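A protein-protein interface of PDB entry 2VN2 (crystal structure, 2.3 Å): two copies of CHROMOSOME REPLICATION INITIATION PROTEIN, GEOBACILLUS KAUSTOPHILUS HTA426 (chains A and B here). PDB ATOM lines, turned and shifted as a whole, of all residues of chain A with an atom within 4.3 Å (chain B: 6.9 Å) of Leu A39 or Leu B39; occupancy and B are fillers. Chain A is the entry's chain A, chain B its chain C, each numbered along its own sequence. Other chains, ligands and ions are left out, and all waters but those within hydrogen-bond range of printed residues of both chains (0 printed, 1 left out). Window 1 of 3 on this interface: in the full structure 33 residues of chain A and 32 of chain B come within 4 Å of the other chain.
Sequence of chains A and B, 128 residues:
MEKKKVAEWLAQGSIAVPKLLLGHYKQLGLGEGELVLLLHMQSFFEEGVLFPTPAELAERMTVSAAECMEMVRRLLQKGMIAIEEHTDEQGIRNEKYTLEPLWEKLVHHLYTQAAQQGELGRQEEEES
O of Val A17 lies within hydrogen-bond range of N of Ile B15.
NE2 of His B40 lies within hydrogen-bond range of O of Arg B60 (3.5 Å).
Of the 11 printed residues of chain A, 6 touch a printed residue of chain B. Printed residues of chain A that touch a printed residue of chain B: Val A17, Leu A22, Val A36, Leu A39, His A40 and Ser A43. Hydrophobic or aromatic side chains of chain A that line the printed part of chain B: Val A17, Leu A22, Val A36, Leu A39 and His A40. Printed residues of chain B that touch a printed residue of chain A: Ile B15, Val B17, Leu B22, Leu B35, Val B36, Leu B39, His B40 and Ser B43. Among the printed residues, 12 pairs touch across the chains. Among the printed residues, no Asp or Glu carboxylate lies within 4 Å of a Lys or Arg side-chain nitrogen of the other chain.
Of chain B, only Leu B22 (3.8 Å) and Leu B39 (3.8 Å) come within 4 Å of Leu A39. Of chain A, only Leu A22 (3.8 Å) and Leu A39 (3.8 Å) come within 4 Å of Leu B39. Of the printed residues of chain B, Leu A22 touches Ile B15 (3.5 Å), Leu B39 (3.8 Å), His B40 (3.3 Å) and Ser B43 (3.97 Å). Printed residues of chain B within 4 Å of Ser A43: Leu B22 (3.9 Å). Of the printed residues of chain A, Val B36 touches Val A36. Of the printed residues of chain A, Ile B15 touches Val A17 and Leu A22. Leu B38 touches none of the printed residues of chain A. Leu B37 touches none of the printed residues of chain A. The nearest residue of chain B that does not touch Leu A39 is Val B17 (4.9 Å). The nearest printed residue of chain A that does not touch Leu B39 is Val A17 (4.5 Å).
Val B17 touches its own counterpart, Val A17. Leu A22 touches His B40, and with the chains exchanged His A40 touches Leu B22. Leu A22 touches Ser B43, and with the chains exchanged Ser A43 touches Leu B22. Val B36 touches its own counterpart, Val A36. Positions printed for both chains: 17, 22, 35, 36, 37, 38, 39, 40, 41, 42 and 43.
Among the printed residues, pairs that only touch across the chains: Val A17 with Val B17 (3.6 Å), Leu A22 with Ile B15 (3.5 Å), Leu A22 with Leu B39 (3.8 Å), Leu A22 with His B40 (3.3 Å), Leu A22 with Ser B43 (3.97 Å), Val A36 with Leu B35 (3.8 Å), Val A36 with Val B36 (3.6 Å), Leu A39 with Leu B22 (3.8 Å), Leu A39 with Leu B39 (3.8 Å), His A40 with Leu B22 (3.2 Å) and Ser A43 with Leu B22 (3.9 Å).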
ATOM      1  N   VAL A  17      19.716  27.489   3.468  1.00  0.00           N
ATOM      2  CA  VAL A  17      20.470  26.542   2.711  1.00  0.00           C
ATOM      3  C   VAL A  17      19.707  25.209   2.664  1.00  0.00           C
ATOM      4  O   VAL A  17      19.598  24.506   3.669  1.00  0.00           O
ATOM      5  CB  VAL A  17      21.802  26.315   3.367  1.00  0.00           C
ATOM      6  CG1 VAL A  17      22.577  25.173   2.720  1.00  0.00           C
ATOM      7  CG2 VAL A  17      22.645  27.614   3.247  1.00  0.00           C
ATOM      8  N   LEU A  22      22.970  20.642   0.757  1.00  0.00           N
ATOM      9  CA  LEU A  22      23.900  20.187   1.775  1.00  0.00           C
ATOM     10  C   LEU A  22      24.098  18.708   1.797  1.00  0.00           C
ATOM     11  O   LEU A  22      25.192  18.244   1.962  1.00  0.00           O
ATOM     12  CB  LEU A  22      23.308  20.622   3.111  1.00  0.00           C
ATOM     13  CG  LEU A  22      24.263  20.705   4.235  1.00  0.00           C
ATOM     14  CD1 LEU A  22      25.361  21.616   3.864  1.00  0.00           C
ATOM     15  CD2 LEU A  22      23.459  21.258   5.415  1.00  0.00           C
ATOM     16  N   LEU A  35      30.427  25.319  -2.742  1.00  0.00           N
ATOM     17  CA  LEU A  35      29.167  25.485  -2.008  1.00  0.00           C
ATOM     18  C   LEU A  35      29.094  26.924  -1.391  1.00  0.00           C
ATOM     19  O   LEU A  35      28.180  27.720  -1.730  1.00  0.00           O
ATOM     20  CB  LEU A  35      28.933  24.345  -0.988  1.00  0.00           C
ATOM     21  CG  LEU A  35      27.559  24.543  -0.363  1.00  0.00           C
ATOM     22  CD1 LEU A  35      26.427  24.061  -1.301  1.00  0.00           C
ATOM     23  CD2 LEU A  35      27.508  23.686   0.859  1.00  0.00           C
ATOM     24  N   VAL A  36      30.087  27.293  -0.556  1.00  0.00           N
ATOM     25  CA  VAL A  36      30.097  28.595   0.039  1.00  0.00           C
ATOM     26  C   VAL A  36      30.052  29.675  -1.073  1.00  0.00           C
ATOM     27  O   VAL A  36      29.434  30.712  -0.903  1.00  0.00           O
ATOM     28  CB  VAL A  36      31.289  28.756   0.994  1.00  0.00           C
ATOM     29  CG1 VAL A  36      31.258  30.262   1.700  1.00  0.00           C
ATOM     30  CG2 VAL A  36      31.280  27.665   2.051  1.00  0.00           C
ATOM     31  N   LEU A  37      30.719  29.450  -2.230  1.00  0.00           N
ATOM     32  CA  LEU A  37      30.677  30.489  -3.290  1.00  0.00           C
ATOM     33  C   LEU A  37      29.207  30.694  -3.739  1.00  0.00           C
ATOM     34  O   LEU A  37      28.746  31.826  -3.895  1.00  0.00           O
ATOM     35  CB  LEU A  37      31.630  30.182  -4.501  1.00  0.00           C
ATOM     36  CG  LEU A  37      31.590  31.208  -5.689  1.00  0.00           C
ATOM     37  CD1 LEU A  37      32.732  31.001  -6.574  1.00  0.00           C
ATOM     38  CD2 LEU A  37      30.342  30.933  -6.584  1.00  0.00           C
ATOM     39  N   LEU A  38      28.487  29.610  -3.926  1.00  0.00           N
ATOM     40  CA  LEU A  38      27.055  29.612  -4.313  1.00  0.00           C
ATOM     41  C   LEU A  38      26.218  30.378  -3.267  1.00  0.00           C
ATOM     42  O   LEU A  38      25.282  31.166  -3.600  1.00  0.00           O
ATOM     43  CB  LEU A  38      26.588  28.113  -4.402  1.00  0.00           C
ATOM     44  CG  LEU A  38      27.093  27.376  -5.644  1.00  0.00           C
ATOM     45  CD1 LEU A  38      26.589  25.917  -5.671  1.00  0.00           C
ATOM     46  CD2 LEU A  38      26.835  28.148  -7.017  1.00  0.00           C
ATOM     47  N   LEU A  39      26.544  30.148  -1.980  1.00  0.00           N
ATOM     48  CA  LEU A  39      25.870  30.906  -0.812  1.00  0.00           C
ATOM     49  C   LEU A  39      26.217  32.299  -0.967  1.00  0.00           C
ATOM     50  O   LEU A  39      25.307  33.128  -0.893  1.00  0.00           O
ATOM     51  CB  LEU A  39      26.381  30.459   0.586  1.00  0.00           C
ATOM     52  CG  LEU A  39      25.721  29.169   1.163  1.00  0.00           C
ATOM     53  CD1 LEU A  39      25.089  28.149   0.157  1.00  0.00           C
ATOM     54  CD2 LEU A  39      26.551  28.402   2.285  1.00  0.00           C
ATOM     55  N   HIS A  40      27.530  32.647  -1.168  1.00  0.00           N
ATOM     56  CA  HIS A  40      27.743  34.154  -1.365  1.00  0.00           C
ATOM     57  C   HIS A  40      26.921  34.688  -2.581  1.00  0.00           C
ATOM     58  O   HIS A  40      26.362  35.780  -2.474  1.00  0.00           O
ATOM     59  CB  HIS A  40      29.165  34.646  -1.488  1.00  0.00           C
ATOM     60  CG  HIS A  40      30.020  34.418  -0.283  1.00  0.00           C
ATOM     61  ND1 HIS A  40      29.954  35.189   0.852  1.00  0.00           N
ATOM     62  CD2 HIS A  40      30.974  33.490  -0.048  1.00  0.00           C
ATOM     63  CE1 HIS A  40      30.826  34.745   1.738  1.00  0.00           C
ATOM     64  NE2 HIS A  40      31.454  33.712   1.212  1.00  0.00           N
ATOM     65  N   MET A  41      26.878  33.975  -3.721  1.00  0.00           N
ATOM     66  CA  MET A  41      26.070  34.453  -4.847  1.00  0.00           C
ATOM     67  C   MET A  41      24.658  34.554  -4.466  1.00  0.00           C
ATOM     68  O   MET A  41      24.112  35.534  -4.776  1.00  0.00           O
ATOM     69  CB  MET A  41      26.097  33.649  -6.141  1.00  0.00           C
ATOM     70  CG  MET A  41      27.533  33.555  -6.876  1.00  0.00           C
ATOM     71  SD  MET A  41      27.591  32.189  -8.160  1.00  0.00           S
ATOM     72  CE  MET A  41      25.977  32.460  -8.731  1.00  0.00           C
ATOM     73  N   GLN A  42      24.064  33.571  -3.792  1.00  0.00           N
ATOM     74  CA  GLN A  42      22.639  33.709  -3.367  1.00  0.00           C
ATOM     75  C   GLN A  42      22.413  35.026  -2.595  1.00  0.00           C
ATOM     76  O   GLN A  42      21.474  35.778  -2.821  1.00  0.00           O
ATOM     77  CB  GLN A  42      22.180  32.541  -2.515  1.00  0.00           C
ATOM     78  CG  GLN A  42      20.672  32.602  -2.181  1.00  0.00           C
ATOM     79  CD  GLN A  42      20.287  31.579  -1.099  1.00  0.00           C
ATOM     80  OE1 GLN A  42      20.981  30.508  -0.912  1.00  0.00           O
ATOM     81  NE2 GLN A  42      19.204  31.909  -0.309  1.00  0.00           N
ATOM     82  N   SER A  43      23.349  35.304  -1.711  1.00  0.00           N
ATOM     83  CA  SER A  43      23.296  36.453  -0.819  1.00  0.00           C
ATOM     84  C   SER A  43      23.321  37.808  -1.559  1.00  0.00           C
ATOM     85  O   SER A  43      22.620  38.742  -1.183  1.00  0.00           O
ATOM     86  CB  SER A  43      24.506  36.337   0.118  1.00  0.00           C
ATOM     87  OG  SER A  43      24.508  37.373   1.061  1.00  0.00           O
ATOM     88  N   ILE B  15      18.893  24.785   6.245  1.00  0.00           N
ATOM     89  CA  ILE B  15      19.651  25.310   7.382  1.00  0.00           C
ATOM     90  C   ILE B  15      19.758  26.854   7.180  1.00  0.00           C
ATOM     91  O   ILE B  15      20.129  27.304   6.129  1.00  0.00           O
ATOM     92  CB  ILE B  15      21.068  24.557   7.413  1.00  0.00           C
ATOM     93  CG1 ILE B  15      20.872  23.264   8.161  1.00  0.00           C
ATOM     94  CG2 ILE B  15      22.203  25.292   8.110  1.00  0.00           C
ATOM     95  CD1 ILE B  15      20.664  22.077   7.276  1.00  0.00           C
ATOM     96  N   ALA B  16      19.453  27.645   8.205  1.00  0.00           N
ATOM     97  CA  ALA B  16      19.479  29.122   8.117  1.00  0.00           C
ATOM     98  C   ALA B  16      20.882  29.561   8.460  1.00  0.00           C
ATOM     99  O   ALA B  16      21.368  29.286   9.565  1.00  0.00           O
ATOM    100  CB  ALA B  16      18.530  29.716   9.147  1.00  0.00           C
ATOM    101  N   VAL B  17      21.513  30.251   7.533  1.00  0.00           N
ATOM    102  CA  VAL B  17      22.862  30.679   7.709  1.00  0.00           C
ATOM    103  C   VAL B  17      22.738  32.201   7.915  1.00  0.00           C
ATOM    104  O   VAL B  17      22.549  32.905   6.929  1.00  0.00           O
ATOM    105  CB  VAL B  17      23.742  30.298   6.413  1.00  0.00           C
ATOM    106  CG1 VAL B  17      25.161  30.941   6.442  1.00  0.00           C
ATOM    107  CG2 VAL B  17      23.953  28.814   6.415  1.00  0.00           C
ATOM    108  N   LEU B  21      27.178  35.761   9.687  1.00  0.00           N
ATOM    109  CA  LEU B  21      28.159  34.752   9.611  1.00  0.00           C
ATOM    110  C   LEU B  21      28.756  34.645   8.191  1.00  0.00           C
ATOM    111  O   LEU B  21      30.019  34.685   8.022  1.00  0.00           O
ATOM    112  CB  LEU B  21      27.672  33.385  10.092  1.00  0.00           C
ATOM    113  CG  LEU B  21      28.641  32.198  10.205  1.00  0.00           C
ATOM    114  CD1 LEU B  21      29.900  32.602  11.082  1.00  0.00           C
ATOM    115  CD2 LEU B  21      27.863  31.010  10.815  1.00  0.00           C
ATOM    116  N   LEU B  22      27.923  34.480   7.169  1.00  0.00           N
ATOM    117  CA  LEU B  22      28.462  34.433   5.774  1.00  0.00           C
ATOM    118  C   LEU B  22      29.439  35.585   5.499  1.00  0.00           C
ATOM    119  O   LEU B  22      30.491  35.406   4.891  1.00  0.00           O
ATOM    120  CB  LEU B  22      27.323  34.601   4.834  1.00  0.00           C
ATOM    121  CG  LEU B  22      27.467  33.987   3.468  1.00  0.00           C
ATOM    122  CD1 LEU B  22      28.149  32.566   3.509  1.00  0.00           C
ATOM    123  CD2 LEU B  22      26.061  34.004   2.760  1.00  0.00           C
ATOM    124  N   GLU B  34      35.470  24.813   6.865  1.00  0.00           N
ATOM    125  CA  GLU B  34      35.092  24.766   8.273  1.00  0.00           C
ATOM    126  C   GLU B  34      33.650  25.305   8.337  1.00  0.00           C
ATOM    127  O   GLU B  34      32.788  24.620   8.886  1.00  0.00           O
ATOM    128  CB  GLU B  34      36.039  25.589   9.176  1.00  0.00           C
ATOM    129  CG  GLU B  34      37.461  24.944   9.501  1.00  0.00           C
ATOM    130  CD  GLU B  34      38.421  26.030  10.034  1.00  0.00           C
ATOM    131  OE1 GLU B  34      38.495  27.162   9.473  1.00  0.00           O
ATOM    132  OE2 GLU B  34      39.087  25.814  11.053  1.00  0.00           O
ATOM    133  N   LEU B  35      33.383  26.441   7.706  1.00  0.00           N
ATOM    134  CA  LEU B  35      32.012  26.911   7.510  1.00  0.00           C
ATOM    135  C   LEU B  35      31.012  25.755   7.134  1.00  0.00           C
ATOM    136  O   LEU B  35      30.031  25.479   7.897  1.00  0.00           O
ATOM    137  CB  LEU B  35      31.930  28.126   6.538  1.00  0.00           C
ATOM    138  CG  LEU B  35      30.531  28.726   6.379  1.00  0.00           C
ATOM    139  CD1 LEU B  35      30.074  29.297   7.810  1.00  0.00           C
ATOM    140  CD2 LEU B  35      30.504  29.892   5.379  1.00  0.00           C
ATOM    141  N   VAL B  36      31.314  25.004   6.048  1.00  0.00           N
ATOM    142  CA  VAL B  36      30.456  23.861   5.666  1.00  0.00           C
ATOM    143  C   VAL B  36      30.331  22.801   6.728  1.00  0.00           C
ATOM    144  O   VAL B  36      29.223  22.268   7.055  1.00  0.00           O
ATOM    145  CB  VAL B  36      30.824  23.261   4.294  1.00  0.00           C
ATOM    146  CG1 VAL B  36      29.921  22.101   4.065  1.00  0.00           C
ATOM    147  CG2 VAL B  36      30.653  24.307   3.273  1.00  0.00           C
ATOM    148  N   LEU B  37      31.460  22.491   7.327  1.00  0.00           N
ATOM    149  CA  LEU B  37      31.479  21.535   8.431  1.00  0.00           C
ATOM    150  C   LEU B  37      30.494  22.011   9.538  1.00  0.00           C
ATOM    151  O   LEU B  37      29.732  21.171  10.082  1.00  0.00           O
ATOM    152  CB  LEU B  37      32.922  21.420   9.004  1.00  0.00           C
ATOM    153  CG  LEU B  37      33.094  20.474  10.262  1.00  0.00           C
ATOM    154  CD1 LEU B  37      32.591  19.043   9.874  1.00  0.00           C
ATOM    155  CD2 LEU B  37      34.586  20.287  10.781  1.00  0.00           C
ATOM    156  N   LEU B  38      30.528  23.310   9.885  1.00  0.00           N
ATOM    157  CA  LEU B  38      29.497  23.934  10.871  1.00  0.00           C
ATOM    158  C   LEU B  38      28.040  23.785  10.339  1.00  0.00           C
ATOM    159  O   LEU B  38      27.110  23.553  11.106  1.00  0.00           O
ATOM    160  CB  LEU B  38      29.799  25.442  11.121  1.00  0.00           C
ATOM    161  CG  LEU B  38      31.176  25.820  11.788  1.00  0.00           C
ATOM    162  CD1 LEU B  38      31.501  27.278  11.805  1.00  0.00           C
ATOM    163  CD2 LEU B  38      31.309  25.293  13.231  1.00  0.00           C
ATOM    164  N   LEU B  39      27.823  23.840   9.003  1.00  0.00           N
ATOM    165  CA  LEU B  39      26.457  23.625   8.467  1.00  0.00           C
ATOM    166  C   LEU B  39      26.045  22.175   8.604  1.00  0.00           C
ATOM    167  O   LEU B  39      24.938  21.895   8.902  1.00  0.00           O
ATOM    168  CB  LEU B  39      26.355  24.082   6.947  1.00  0.00           C
ATOM    169  CG  LEU B  39      26.842  25.540   6.610  1.00  0.00           C
ATOM    170  CD1 LEU B  39      26.410  26.001   5.180  1.00  0.00           C
ATOM    171  CD2 LEU B  39      26.383  26.546   7.672  1.00  0.00           C
ATOM    172  N   HIS B  40      26.927  21.247   8.301  1.00  0.00           N
ATOM    173  CA  HIS B  40      26.637  19.809   8.511  1.00  0.00           C
ATOM    174  C   HIS B  40      26.349  19.453  10.006  1.00  0.00           C
ATOM    175  O   HIS B  40      25.393  18.734  10.269  1.00  0.00           O
ATOM    176  CB  HIS B  40      27.813  18.960   8.031  1.00  0.00           C
ATOM    177  CG  HIS B  40      27.929  18.881   6.558  1.00  0.00           C
ATOM    178  ND1 HIS B  40      26.865  18.553   5.747  1.00  0.00           N
ATOM    179  CD2 HIS B  40      28.994  19.036   5.743  1.00  0.00           C
ATOM    180  CE1 HIS B  40      27.272  18.506   4.488  1.00  0.00           C
ATOM    181  NE2 HIS B  40      28.548  18.869   4.457  1.00  0.00           N
ATOM    182  N   MET B  41      27.152  19.993  10.945  1.00  0.00           N
ATOM    183  CA  MET B  41      26.868  19.878  12.452  1.00  0.00           C
ATOM    184  C   MET B  41      25.478  20.364  12.794  1.00  0.00           C
ATOM    185  O   MET B  41      24.746  19.662  13.430  1.00  0.00           O
ATOM    186  CB  MET B  41      27.823  20.729  13.301  1.00  0.00           C
ATOM    187  CG  MET B  41      28.718  20.108  14.527  1.00  0.00           C
ATOM    188  SD  MET B  41      30.342  21.021  14.424  1.00  0.00           S
ATOM    189  CE  MET B  41      31.453  19.675  14.518  1.00  0.00           C
ATOM    190  N   GLN B  42      25.108  21.558  12.348  1.00  0.00           N
ATOM    191  CA  GLN B  42      23.745  22.171  12.614  1.00  0.00           C
ATOM    192  C   GLN B  42      22.667  21.241  12.113  1.00  0.00           C
ATOM    193  O   GLN B  42      21.634  20.987  12.744  1.00  0.00           O
ATOM    194  CB  GLN B  42      23.630  23.560  11.901  1.00  0.00           C
ATOM    195  CG  GLN B  42      22.373  24.374  12.204  1.00  0.00           C
ATOM    196  CD  GLN B  42      22.132  24.636  13.719  1.00  0.00           C
ATOM    197  OE1 GLN B  42      23.058  25.021  14.422  1.00  0.00           O
ATOM    198  NE2 GLN B  42      20.873  24.513  14.183  1.00  0.00           N
ATOM    199  N   SER B  43      22.936  20.685  10.942  1.00  0.00           N
ATOM    200  CA  SER B  43      21.998  19.813  10.310  1.00  0.00           C
ATOM    201  C   SER B  43      21.877  18.490  11.053  1.00  0.00           C
ATOM    202  O   SER B  43      20.764  17.919  11.220  1.00  0.00           O
ATOM    203  CB  SER B  43      22.557  19.627   8.915  1.00  0.00           C
ATOM    204  OG  SER B  43      21.628  18.979   8.216  1.00  0.00           O
ATOM    205  N   PHE B  44      23.016  17.937  11.508  1.00  0.00           N
ATOM    206  CA  PHE B  44      22.886  16.729  12.392  1.00  0.00           C
ATOM    207  C   PHE B  44      22.027  17.090  13.635  1.00  0.00           C
ATOM    208  O   PHE B  44      21.175  16.349  14.014  1.00  0.00           O
ATOM    209  CB  PHE B  44      24.243  16.107  12.827  1.00  0.00           C
ATOM    210  CG  PHE B  44      24.767  15.145  11.860  1.00  0.00           C
ATOM    211  CD1 PHE B  44      24.227  13.894  11.771  1.00  0.00           C
ATOM    212  CD2 PHE B  44      25.758  15.521  10.942  1.00  0.00           C
ATOM    213  CE1 PHE B  44      24.659  13.028  10.816  1.00  0.00           C
ATOM    214  CE2 PHE B  44      26.249  14.623   9.969  1.00  0.00           C
ATOM    215  CZ  PHE B  44      25.722  13.375   9.923  1.00  0.00           C
ATOM    216  N   LEU B  57      30.232  13.250   9.879  1.00  0.00           N
ATOM    217  CA  LEU B  57      30.451  14.548   9.318  1.00  0.00           C
ATOM    218  C   LEU B  57      31.093  14.483   7.962  1.00  0.00           C
ATOM    219  O   LEU B  57      30.570  15.114   7.030  1.00  0.00           O
ATOM    220  CB  LEU B  57      31.226  15.459  10.267  1.00  0.00           C
ATOM    221  CG  LEU B  57      30.472  15.810  11.533  1.00  0.00           C
ATOM    222  CD1 LEU B  57      31.346  16.246  12.760  1.00  0.00           C
ATOM    223  CD2 LEU B  57      29.473  16.921  11.264  1.00  0.00           C
ATOM    224  N   ARG B  60      29.454  13.422   4.175  1.00  0.00           N
ATOM    225  CA  ARG B  60      28.754  14.369   3.396  1.00  0.00           C
ATOM    226  C   ARG B  60      29.676  15.404   2.880  1.00  0.00           C
ATOM    227  O   ARG B  60      29.212  16.307   2.236  1.00  0.00           O
ATOM    228  CB  ARG B  60      27.514  14.833   4.196  1.00  0.00           C
ATOM    229  CG  ARG B  60      26.245  14.072   3.593  1.00  0.00           C
ATOM    230  CD  ARG B  60      25.284  13.357   4.553  1.00  0.00           C
ATOM    231  NE  ARG B  60      25.088  13.989   5.884  1.00  0.00           N
ATOM    232  CZ  ARG B  60      24.148  14.925   6.183  1.00  0.00           C
ATOM    233  NH1 ARG B  60      23.328  15.396   5.220  1.00  0.00           N
ATOM    234  NH2 ARG B  60      24.017  15.431   7.437  1.00  0.00           N
ATOM    235  N   LEU B  99      27.541  25.489  19.223  1.00  0.00           N
ATOM    236  CA  LEU B  99      28.135  26.640  18.464  1.00  0.00           C
ATOM    237  C   LEU B  99      28.064  27.977  19.227  1.00  0.00           C
ATOM    238  O   LEU B  99      28.613  28.991  18.842  1.00  0.00           O
ATOM    239  CB  LEU B  99      27.382  26.793  17.137  1.00  0.00           C
ATOM    240  CG  LEU B  99      27.741  25.940  15.886  1.00  0.00           C
ATOM    241  CD1 LEU B  99      28.311  24.524  16.163  1.00  0.00           C
ATOM    242  CD2 LEU B  99      26.462  25.846  14.831  1.00  0.00           C
